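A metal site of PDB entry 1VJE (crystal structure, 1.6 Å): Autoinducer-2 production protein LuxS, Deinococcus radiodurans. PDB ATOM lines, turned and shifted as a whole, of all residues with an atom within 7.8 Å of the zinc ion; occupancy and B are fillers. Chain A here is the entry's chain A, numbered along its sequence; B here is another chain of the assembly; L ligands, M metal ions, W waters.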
ATOM      1  N   HIS A  57      14.024 -24.205 -26.289  1.00  0.00           N
ATOM      2  CA  HIS A  57      12.720 -24.861 -26.479  1.00  0.00           C
ATOM      3  C   HIS A  57      12.959 -26.181 -27.192  1.00  0.00           C
ATOM      4  O   HIS A  57      12.448 -27.244 -26.801  1.00  0.00           O
ATOM      5  CB  HIS A  57      11.806 -23.932 -27.286  1.00  0.00           C
ATOM      6  CG  HIS A  57      10.379 -24.431 -27.382  1.00  0.00           C
ATOM      7  ND1 HIS A  57       9.583 -23.914 -28.391  1.00  0.00           N
ATOM      8  CD2 HIS A  57       9.649 -25.343 -26.729  1.00  0.00           C
ATOM      9  CE1 HIS A  57       8.375 -24.457 -28.295  1.00  0.00           C
ATOM     10  NE2 HIS A  57       8.370 -25.308 -27.290  1.00  0.00           N
ATOM     11  N   THR A  58      13.821 -26.197 -28.216  1.00  0.00           N
ATOM     12  CA  THR A  58      14.168 -27.466 -28.884  1.00  0.00           C
ATOM     13  C   THR A  58      14.927 -28.398 -27.954  1.00  0.00           C
ATOM     14  O   THR A  58      14.626 -29.602 -27.894  1.00  0.00           O
ATOM     15  CB  THR A  58      14.936 -27.182 -30.195  1.00  0.00           C
ATOM     16  OG1 THR A  58      14.085 -26.369 -31.013  1.00  0.00           O
ATOM     17  CG2 THR A  58      15.220 -28.522 -30.867  1.00  0.00           C
ATOM     18  N   GLU A  60      14.592 -28.580 -24.824  1.00  0.00           N
ATOM     19  CA  GLU A  60      13.559 -29.128 -23.930  1.00  0.00           C
ATOM     20  C   GLU A  60      12.823 -30.292 -24.605  1.00  0.00           C
ATOM     21  O   GLU A  60      12.649 -31.337 -23.996  1.00  0.00           O
ATOM     22  CB  GLU A  60      12.538 -28.028 -23.641  1.00  0.00           C
ATOM     23  CG  GLU A  60      11.372 -28.432 -22.751  1.00  0.00           C
ATOM     24  CD  GLU A  60      10.271 -27.411 -22.803  1.00  0.00           C
ATOM     25  OE1 GLU A  60       9.848 -27.012 -23.925  1.00  0.00           O
ATOM     26  OE2 GLU A  60       9.800 -26.968 -21.739  1.00  0.00           O
ATOM     27  N   HIS A  61      12.397 -30.113 -25.846  1.00  0.00           N
ATOM     28  CA  HIS A  61      11.691 -31.237 -26.501  1.00  0.00           C
ATOM     29  C   HIS A  61      12.576 -32.456 -26.641  1.00  0.00           C
ATOM     30  O   HIS A  61      12.118 -33.575 -26.431  1.00  0.00           O
ATOM     31  CB  HIS A  61      11.284 -30.749 -27.914  1.00  0.00           C
ATOM     32  CG  HIS A  61      10.004 -29.986 -27.939  1.00  0.00           C
ATOM     33  ND1 HIS A  61       8.994 -30.289 -28.846  1.00  0.00           N
ATOM     34  CD2 HIS A  61       9.575 -28.903 -27.222  1.00  0.00           C
ATOM     35  CE1 HIS A  61       7.998 -29.439 -28.668  1.00  0.00           C
ATOM     36  NE2 HIS A  61       8.321 -28.599 -27.705  1.00  0.00           N
ATOM     37  N   ILE A 117      12.164 -32.543 -35.202  1.00  0.00           N
ATOM     38  CA  ILE A 117      12.062 -32.369 -33.706  1.00  0.00           C
ATOM     39  C   ILE A 117      10.753 -32.993 -33.286  1.00  0.00           C
ATOM     40  O   ILE A 117       9.696 -32.639 -33.861  1.00  0.00           O
ATOM     41  CB  ILE A 117      12.033 -30.881 -33.367  1.00  0.00           C
ATOM     42  CG1 ILE A 117      13.244 -30.077 -33.868  1.00  0.00           C
ATOM     43  CG2 ILE A 117      11.991 -30.700 -31.824  1.00  0.00           C
ATOM     44  CD1 ILE A 117      12.972 -28.572 -33.831  1.00  0.00           C
ATOM     45  N   PRO A 118      10.713 -33.821 -32.260  1.00  0.00           N
ATOM     46  CA  PRO A 118       9.497 -34.437 -31.785  1.00  0.00           C
ATOM     47  C   PRO A 118       8.574 -33.386 -31.166  1.00  0.00           C
ATOM     48  O   PRO A 118       9.076 -32.389 -30.629  1.00  0.00           O
ATOM     49  CB  PRO A 118       9.935 -35.420 -30.705  1.00  0.00           C
ATOM     50  CG  PRO A 118      11.309 -35.015 -30.348  1.00  0.00           C
ATOM     51  CD  PRO A 118      11.924 -34.331 -31.539  1.00  0.00           C
ATOM     52  N   GLY A 119       7.282 -33.595 -31.337  1.00  0.00           N
ATOM     53  CA  GLY A 119       6.280 -32.736 -30.766  1.00  0.00           C
ATOM     54  C   GLY A 119       6.142 -31.344 -31.295  1.00  0.00           C
ATOM     55  O   GLY A 119       5.538 -30.479 -30.623  1.00  0.00           O
ATOM     56  N   VAL A 120       6.588 -31.050 -32.522  1.00  0.00           N
ATOM     57  CA  VAL A 120       6.477 -29.687 -33.041  1.00  0.00           C
ATOM     58  C   VAL A 120       5.271 -29.573 -33.977  1.00  0.00           C
ATOM     59  O   VAL A 120       5.345 -29.935 -35.158  1.00  0.00           O
ATOM     60  CB  VAL A 120       7.756 -29.235 -33.731  1.00  0.00           C
ATOM     61  CG1 VAL A 120       7.660 -27.837 -34.316  1.00  0.00           C
ATOM     62  CG2 VAL A 120       8.941 -29.325 -32.754  1.00  0.00           C
ATOM     63  N   SER A 121       4.178 -29.068 -33.440  1.00  0.00           N
ATOM     64  CA  SER A 121       2.953 -28.872 -34.201  1.00  0.00           C
ATOM     65  C   SER A 121       2.001 -28.024 -33.324  1.00  0.00           C
ATOM     66  O   SER A 121       2.199 -27.976 -32.124  1.00  0.00           O
ATOM     67  CB  SER A 121       2.247 -30.191 -34.495  1.00  0.00           C
ATOM     68  OG  SER A 121       1.810 -30.859 -33.299  1.00  0.00           O
ATOM     69  N   GLU A 124       0.587 -30.349 -30.599  1.00  0.00           N
ATOM     70  CA  GLU A 124       1.396 -30.834 -29.486  1.00  0.00           C
ATOM     71  C   GLU A 124       2.312 -29.879 -28.759  1.00  0.00           C
ATOM     72  O   GLU A 124       2.900 -30.307 -27.729  1.00  0.00           O
ATOM     73  CB  GLU A 124       2.344 -31.939 -30.083  1.00  0.00           C
ATOM     74  CG  GLU A 124       1.612 -33.048 -30.847  1.00  0.00           C
ATOM     75  CD  GLU A 124       2.608 -33.779 -31.756  1.00  0.00           C
ATOM     76  OE1 GLU A 124       3.143 -33.147 -32.702  1.00  0.00           O
ATOM     77  OE2 GLU A 124       2.958 -34.936 -31.466  1.00  0.00           O
ATOM     78  N   CYS A 125       2.443 -28.662 -29.237  1.00  0.00           N
ATOM     79  CA  CYS A 125       3.375 -27.683 -28.684  1.00  0.00           C
ATOM     80  C   CYS A 125       2.709 -26.332 -28.530  1.00  0.00           C
ATOM     81  O   CYS A 125       1.884 -25.954 -29.400  1.00  0.00           O
ATOM     82  CB  CYS A 125       4.518 -27.606 -29.713  1.00  0.00           C
ATOM     83  SG  CYS A 125       5.843 -26.440 -29.318  1.00  0.00           S
ATOM     84  N   GLY A 126       3.002 -25.601 -27.460  1.00  0.00           N
ATOM     85  CA  GLY A 126       2.403 -24.294 -27.233  1.00  0.00           C
ATOM     86  C   GLY A 126       3.021 -23.128 -27.995  1.00  0.00           C
ATOM     87  O   GLY A 126       2.533 -22.005 -27.911  1.00  0.00           O
ATOM     88  N   ASN A 127       4.128 -23.368 -28.695  1.00  0.00           N
ATOM     89  CA  ASN A 127       4.779 -22.316 -29.527  1.00  0.00           C
ATOM     90  C   ASN A 127       5.589 -23.082 -30.593  1.00  0.00           C
ATOM     91  O   ASN A 127       6.816 -23.051 -30.647  1.00  0.00           O
ATOM     92  CB  ASN A 127       5.674 -21.404 -28.706  1.00  0.00           C
ATOM     93  CG  ASN A 127       6.054 -20.123 -29.404  1.00  0.00           C
ATOM     94  OD1 ASN A 127       5.659 -19.900 -30.562  1.00  0.00           O
ATOM     95  ND2 ASN A 127       6.850 -19.270 -28.757  1.00  0.00           N
ATOM     96  N   TYR A 128       4.861 -23.723 -31.521  1.00  0.00           N
ATOM     97  CA  TYR A 128       5.538 -24.580 -32.504  1.00  0.00           C
ATOM     98  C   TYR A 128       6.419 -23.845 -33.502  1.00  0.00           C
ATOM     99  O   TYR A 128       7.304 -24.490 -34.109  1.00  0.00           O
ATOM    100  CB  TYR A 128       4.530 -25.479 -33.213  1.00  0.00           C
ATOM    101  CG  TYR A 128       3.645 -24.743 -34.220  1.00  0.00           C
ATOM    102  CD1 TYR A 128       4.051 -24.559 -35.517  1.00  0.00           C
ATOM    103  CD2 TYR A 128       2.394 -24.287 -33.847  1.00  0.00           C
ATOM    104  CE1 TYR A 128       3.252 -23.899 -36.430  1.00  0.00           C
ATOM    105  CE2 TYR A 128       1.585 -23.592 -34.727  1.00  0.00           C
ATOM    106  CZ  TYR A 128       2.017 -23.431 -36.034  1.00  0.00           C
ATOM    107  OH  TYR A 128       1.223 -22.755 -36.933  1.00  0.00           O
ATOM    108  N   ARG A 129       6.309 -22.538 -33.597  1.00  0.00           N
ATOM    109  CA  ARG A 129       7.155 -21.821 -34.544  1.00  0.00           C
ATOM    110  C   ARG A 129       8.482 -21.406 -33.925  1.00  0.00           C
ATOM    111  O   ARG A 129       9.306 -20.860 -34.658  1.00  0.00           O
ATOM    112  CB  ARG A 129       6.437 -20.578 -35.027  1.00  0.00           C
ATOM    113  CG  ARG A 129       5.121 -20.933 -35.755  1.00  0.00           C
ATOM    114  CD  ARG A 129       4.165 -19.850 -35.301  1.00  0.00           C
ATOM    115  NE  ARG A 129       3.044 -19.592 -36.171  1.00  0.00           N
ATOM    116  CZ  ARG A 129       1.877 -19.229 -35.637  1.00  0.00           C
ATOM    117  NH1 ARG A 129       0.858 -18.992 -36.431  1.00  0.00           N
ATOM    118  NH2 ARG A 129       1.763 -19.154 -34.306  1.00  0.00           N
ATOM    119  N   ASP A 130       8.677 -21.603 -32.641  1.00  0.00           N
ATOM    120  CA  ASP A 130       9.895 -21.144 -31.985  1.00  0.00           C
ATOM    121  C   ASP A 130      10.864 -22.259 -31.651  1.00  0.00           C
ATOM    122  O   ASP A 130      10.971 -22.689 -30.490  1.00  0.00           O
ATOM    123  CB  ASP A 130       9.454 -20.464 -30.653  1.00  0.00           C
ATOM    124  CG  ASP A 130      10.585 -19.628 -30.072  1.00  0.00           C
ATOM    125  OD1 ASP A 130      11.283 -18.931 -30.839  1.00  0.00           O
ATOM    126  OD2 ASP A 130      10.765 -19.671 -28.834  1.00  0.00           O
ATOM    127  N   HIS A 131      11.499 -22.838 -32.650  1.00  0.00           N
ATOM    128  CA  HIS A 131      12.463 -23.908 -32.512  1.00  0.00           C
ATOM    129  C   HIS A 131      13.735 -23.649 -33.302  1.00  0.00           C
ATOM    130  O   HIS A 131      13.719 -22.793 -34.197  1.00  0.00           O
ATOM    131  CB  HIS A 131      11.834 -25.239 -33.009  1.00  0.00           C
ATOM    132  CG  HIS A 131      10.891 -25.797 -31.992  1.00  0.00           C
ATOM    133  ND1 HIS A 131      11.300 -26.443 -30.848  1.00  0.00           N
ATOM    134  CD2 HIS A 131       9.534 -25.736 -31.947  1.00  0.00           C
ATOM    135  CE1 HIS A 131      10.227 -26.783 -30.139  1.00  0.00           C
ATOM    136  NE2 HIS A 131       9.167 -26.378 -30.783  1.00  0.00           N
ATOM    137  N   SER B   9       3.712 -34.597 -22.386  1.00  0.00           N
ATOM    138  CA  SER B   9       3.396 -33.258 -22.825  1.00  0.00           C
ATOM    139  C   SER B   9       2.797 -33.206 -24.242  1.00  0.00           C
ATOM    140  O   SER B   9       1.971 -32.362 -24.507  1.00  0.00           O
ATOM    141  CB  SER B   9       4.563 -32.308 -22.677  1.00  0.00           C
ATOM    142  OG  SER B   9       4.301 -30.964 -22.984  1.00  0.00           O
ATOM    143  N   PHE B  10       3.286 -33.989 -25.127  1.00  0.00           N
ATOM    144  CA  PHE B  10       2.928 -33.915 -26.534  1.00  0.00           C
ATOM    145  C   PHE B  10       1.554 -34.546 -26.802  1.00  0.00           C
ATOM    146  O   PHE B  10       1.069 -34.458 -27.938  1.00  0.00           O
ATOM    147  CB  PHE B  10       3.936 -34.668 -27.410  1.00  0.00           C
ATOM    148  CG  PHE B  10       5.357 -34.168 -27.355  1.00  0.00           C
ATOM    149  CD1 PHE B  10       5.592 -32.822 -27.080  1.00  0.00           C
ATOM    150  CD2 PHE B  10       6.416 -34.999 -27.609  1.00  0.00           C
ATOM    151  CE1 PHE B  10       6.874 -32.328 -27.053  1.00  0.00           C
ATOM    152  CE2 PHE B  10       7.716 -34.520 -27.578  1.00  0.00           C
ATOM    153  CZ  PHE B  10       7.945 -33.182 -27.273  1.00  0.00           C
ATOM    154  N   HIS B  14      -3.352 -29.128 -27.756  1.00  0.00           N
ATOM    155  CA  HIS B  14      -3.157 -27.709 -27.485  1.00  0.00           C
ATOM    156  C   HIS B  14      -4.159 -26.803 -28.184  1.00  0.00           C
ATOM    157  O   HIS B  14      -4.271 -25.628 -27.803  1.00  0.00           O
ATOM    158  CB  HIS B  14      -1.718 -27.263 -27.817  1.00  0.00           C
ATOM    159  CG  HIS B  14      -0.699 -27.809 -26.864  1.00  0.00           C
ATOM    160  ND1 HIS B  14      -0.458 -29.163 -26.736  1.00  0.00           N
ATOM    161  CD2 HIS B  14       0.140 -27.160 -26.011  1.00  0.00           C
ATOM    162  CE1 HIS B  14       0.509 -29.339 -25.823  1.00  0.00           C
ATOM    163  NE2 HIS B  14       0.878 -28.159 -25.393  1.00  0.00           N
ATOM    164  N   ASN B  47       0.014 -21.047 -29.022  1.00  0.00           N
ATOM    165  CA  ASN B  47       0.262 -20.524 -30.355  1.00  0.00           C
ATOM    166  C   ASN B  47      -0.380 -19.230 -30.737  1.00  0.00           C
ATOM    167  O   ASN B  47      -0.445 -18.894 -31.932  1.00  0.00           O
ATOM    168  CB  ASN B  47      -0.026 -21.673 -31.374  1.00  0.00           C
ATOM    169  CG  ASN B  47       0.941 -22.816 -31.090  1.00  0.00           C
ATOM    170  OD1 ASN B  47       2.154 -22.592 -31.220  1.00  0.00           O
ATOM    171  ND2 ASN B  47       0.446 -23.959 -30.652  1.00  0.00           N
ATOM    172  N   MET B  80       7.789 -22.932 -19.010  1.00  0.00           N
ATOM    173  CA  MET B  80       7.749 -23.892 -20.127  1.00  0.00           C
ATOM    174  C   MET B  80       8.597 -23.342 -21.272  1.00  0.00           C
ATOM    175  O   MET B  80       8.608 -22.140 -21.529  1.00  0.00           O
ATOM    176  CB  MET B  80       6.310 -24.065 -20.659  1.00  0.00           C
ATOM    177  CG  MET B  80       5.437 -24.743 -19.603  1.00  0.00           C
ATOM    178  SD  MET B  80       3.739 -24.799 -20.257  1.00  0.00           S
ATOM    179  CE  MET B  80       2.972 -25.754 -18.929  1.00  0.00           C
ATOM    180  N   GLY B  81       9.208 -24.228 -22.067  1.00  0.00           N
ATOM    181  CA  GLY B  81       9.972 -23.789 -23.246  1.00  0.00           C
ATOM    182  C   GLY B  81       9.107 -23.011 -24.231  1.00  0.00           C
ATOM    183  O   GLY B  81       9.564 -22.126 -24.964  1.00  0.00           O
ATOM    184  N   CSD B  82       7.807 -23.371 -24.310  1.00  0.00           N
ATOM    185  CA  CSD B  82       6.899 -22.688 -25.224  1.00  0.00           C
ATOM    186  CB  CSD B  82       5.668 -23.546 -25.463  1.00  0.00           C
ATOM    187  SG  CSD B  82       4.776 -24.115 -23.951  1.00  0.00           S
ATOM    188  C   CSD B  82       6.507 -21.288 -24.763  1.00  0.00           C
ATOM    189  O   CSD B  82       5.845 -20.552 -25.480  1.00  0.00           O
ATOM    190  OD1 CSD B  82       4.309 -22.825 -23.345  1.00  0.00           O
ATOM    191  OD2 CSD B  82       3.625 -24.863 -24.492  1.00  0.00           O
ATOM    192  N   ARG B  83       6.869 -20.943 -23.534  1.00  0.00           N
ATOM    193  CA  ARG B  83       6.667 -19.635 -22.955  1.00  0.00           C
ATOM    194  C   ARG B  83       5.220 -19.179 -22.895  1.00  0.00           C
ATOM    195  O   ARG B  83       4.973 -17.954 -22.936  1.00  0.00           O
ATOM    196  CB  ARG B  83       7.573 -18.577 -23.616  1.00  0.00           C
ATOM    197  CG  ARG B  83       9.037 -18.894 -23.278  1.00  0.00           C
ATOM    198  CD  ARG B  83      10.009 -17.892 -23.859  1.00  0.00           C
ATOM    199  NE  ARG B  83      10.089 -17.975 -25.324  1.00  0.00           N
ATOM    200  CZ  ARG B  83       9.683 -17.079 -26.192  1.00  0.00           C
ATOM    201  NH1 ARG B  83       9.106 -15.931 -25.869  1.00  0.00           N
ATOM    202  NH2 ARG B  83       9.879 -17.300 -27.514  1.00  0.00           N
HETATM  203  N1  LIG L   1       8.933 -30.480 -18.871  1.00  0.00           N
HETATM  204  C1  LIG L   1       8.022 -31.422 -19.573  1.00  0.00           C
HETATM  205  C2  LIG L   1       8.430 -32.844 -19.244  1.00  0.00           C
HETATM  206  O1  LIG L   1       9.568 -33.042 -18.757  1.00  0.00           O
HETATM  207  O2  LIG L   1       7.509 -33.664 -18.898  1.00  0.00           O
HETATM  208  C3  LIG L   1       8.103 -31.053 -21.028  1.00  0.00           C
HETATM  209  C4  LIG L   1       7.948 -32.046 -22.132  1.00  0.00           C
HETATM  210 SE1  LIG L   1       8.621 -31.304 -23.765  1.00  0.00          SE
HETATM  211  C5  LIG L   1       7.507 -29.736 -23.912  1.00  0.00           C
HETATM  212 ZN    ZN M   1       7.042 -26.911 -27.480  1.00  0.00          ZN
HETATM  213  O   HOH W   1       5.675 -27.204 -25.817  1.00  0.00           O
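The zinc ion is bound by NE2 of His 57 (2.1 Å), NE2 of His 61 (2.1 Å), water W1 (2.2 Å) and SG of Cys 125 (2.2 Å).
The side-chain sulfur of Cys 125 sits close to a ring nitrogen (NE2) of His 131 (3.6 Å). A ring nitrogen (ND1) of His 57 lies close to a ring nitrogen (NE2) of His 131 (3.5 Å). N of Asn 127 lies close to SG of Cys 125. A ring nitrogen (ND1) of His 57 is in hydrogen-bond range of the backbone carbonyl oxygen of Asp 130 (2.8 Å). The side-chain hydroxyl of Thr 58 is in hydrogen-bond range of a ring nitrogen (ND1) of His 131 (2.8 Å). N of Tyr 128 sits close to SG of Cys 125, 3.6 Å away. A ring nitrogen (ND1) of His 61 lies within hydrogen-bond range of the backbone carbonyl oxygen (O) of Pro 118 (2.8 Å). The side-chain amide nitrogen (ND2) of Asn 47 of chain B sits at hydrogen-bond distance from the backbone carbonyl oxygen (O) of Cys 125 (2.8 Å).
Residues that only touch the zinc ion: His 131 (3.96 Å). Of the 25 residues printed, 4 come within 4 Å of the zinc ion.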
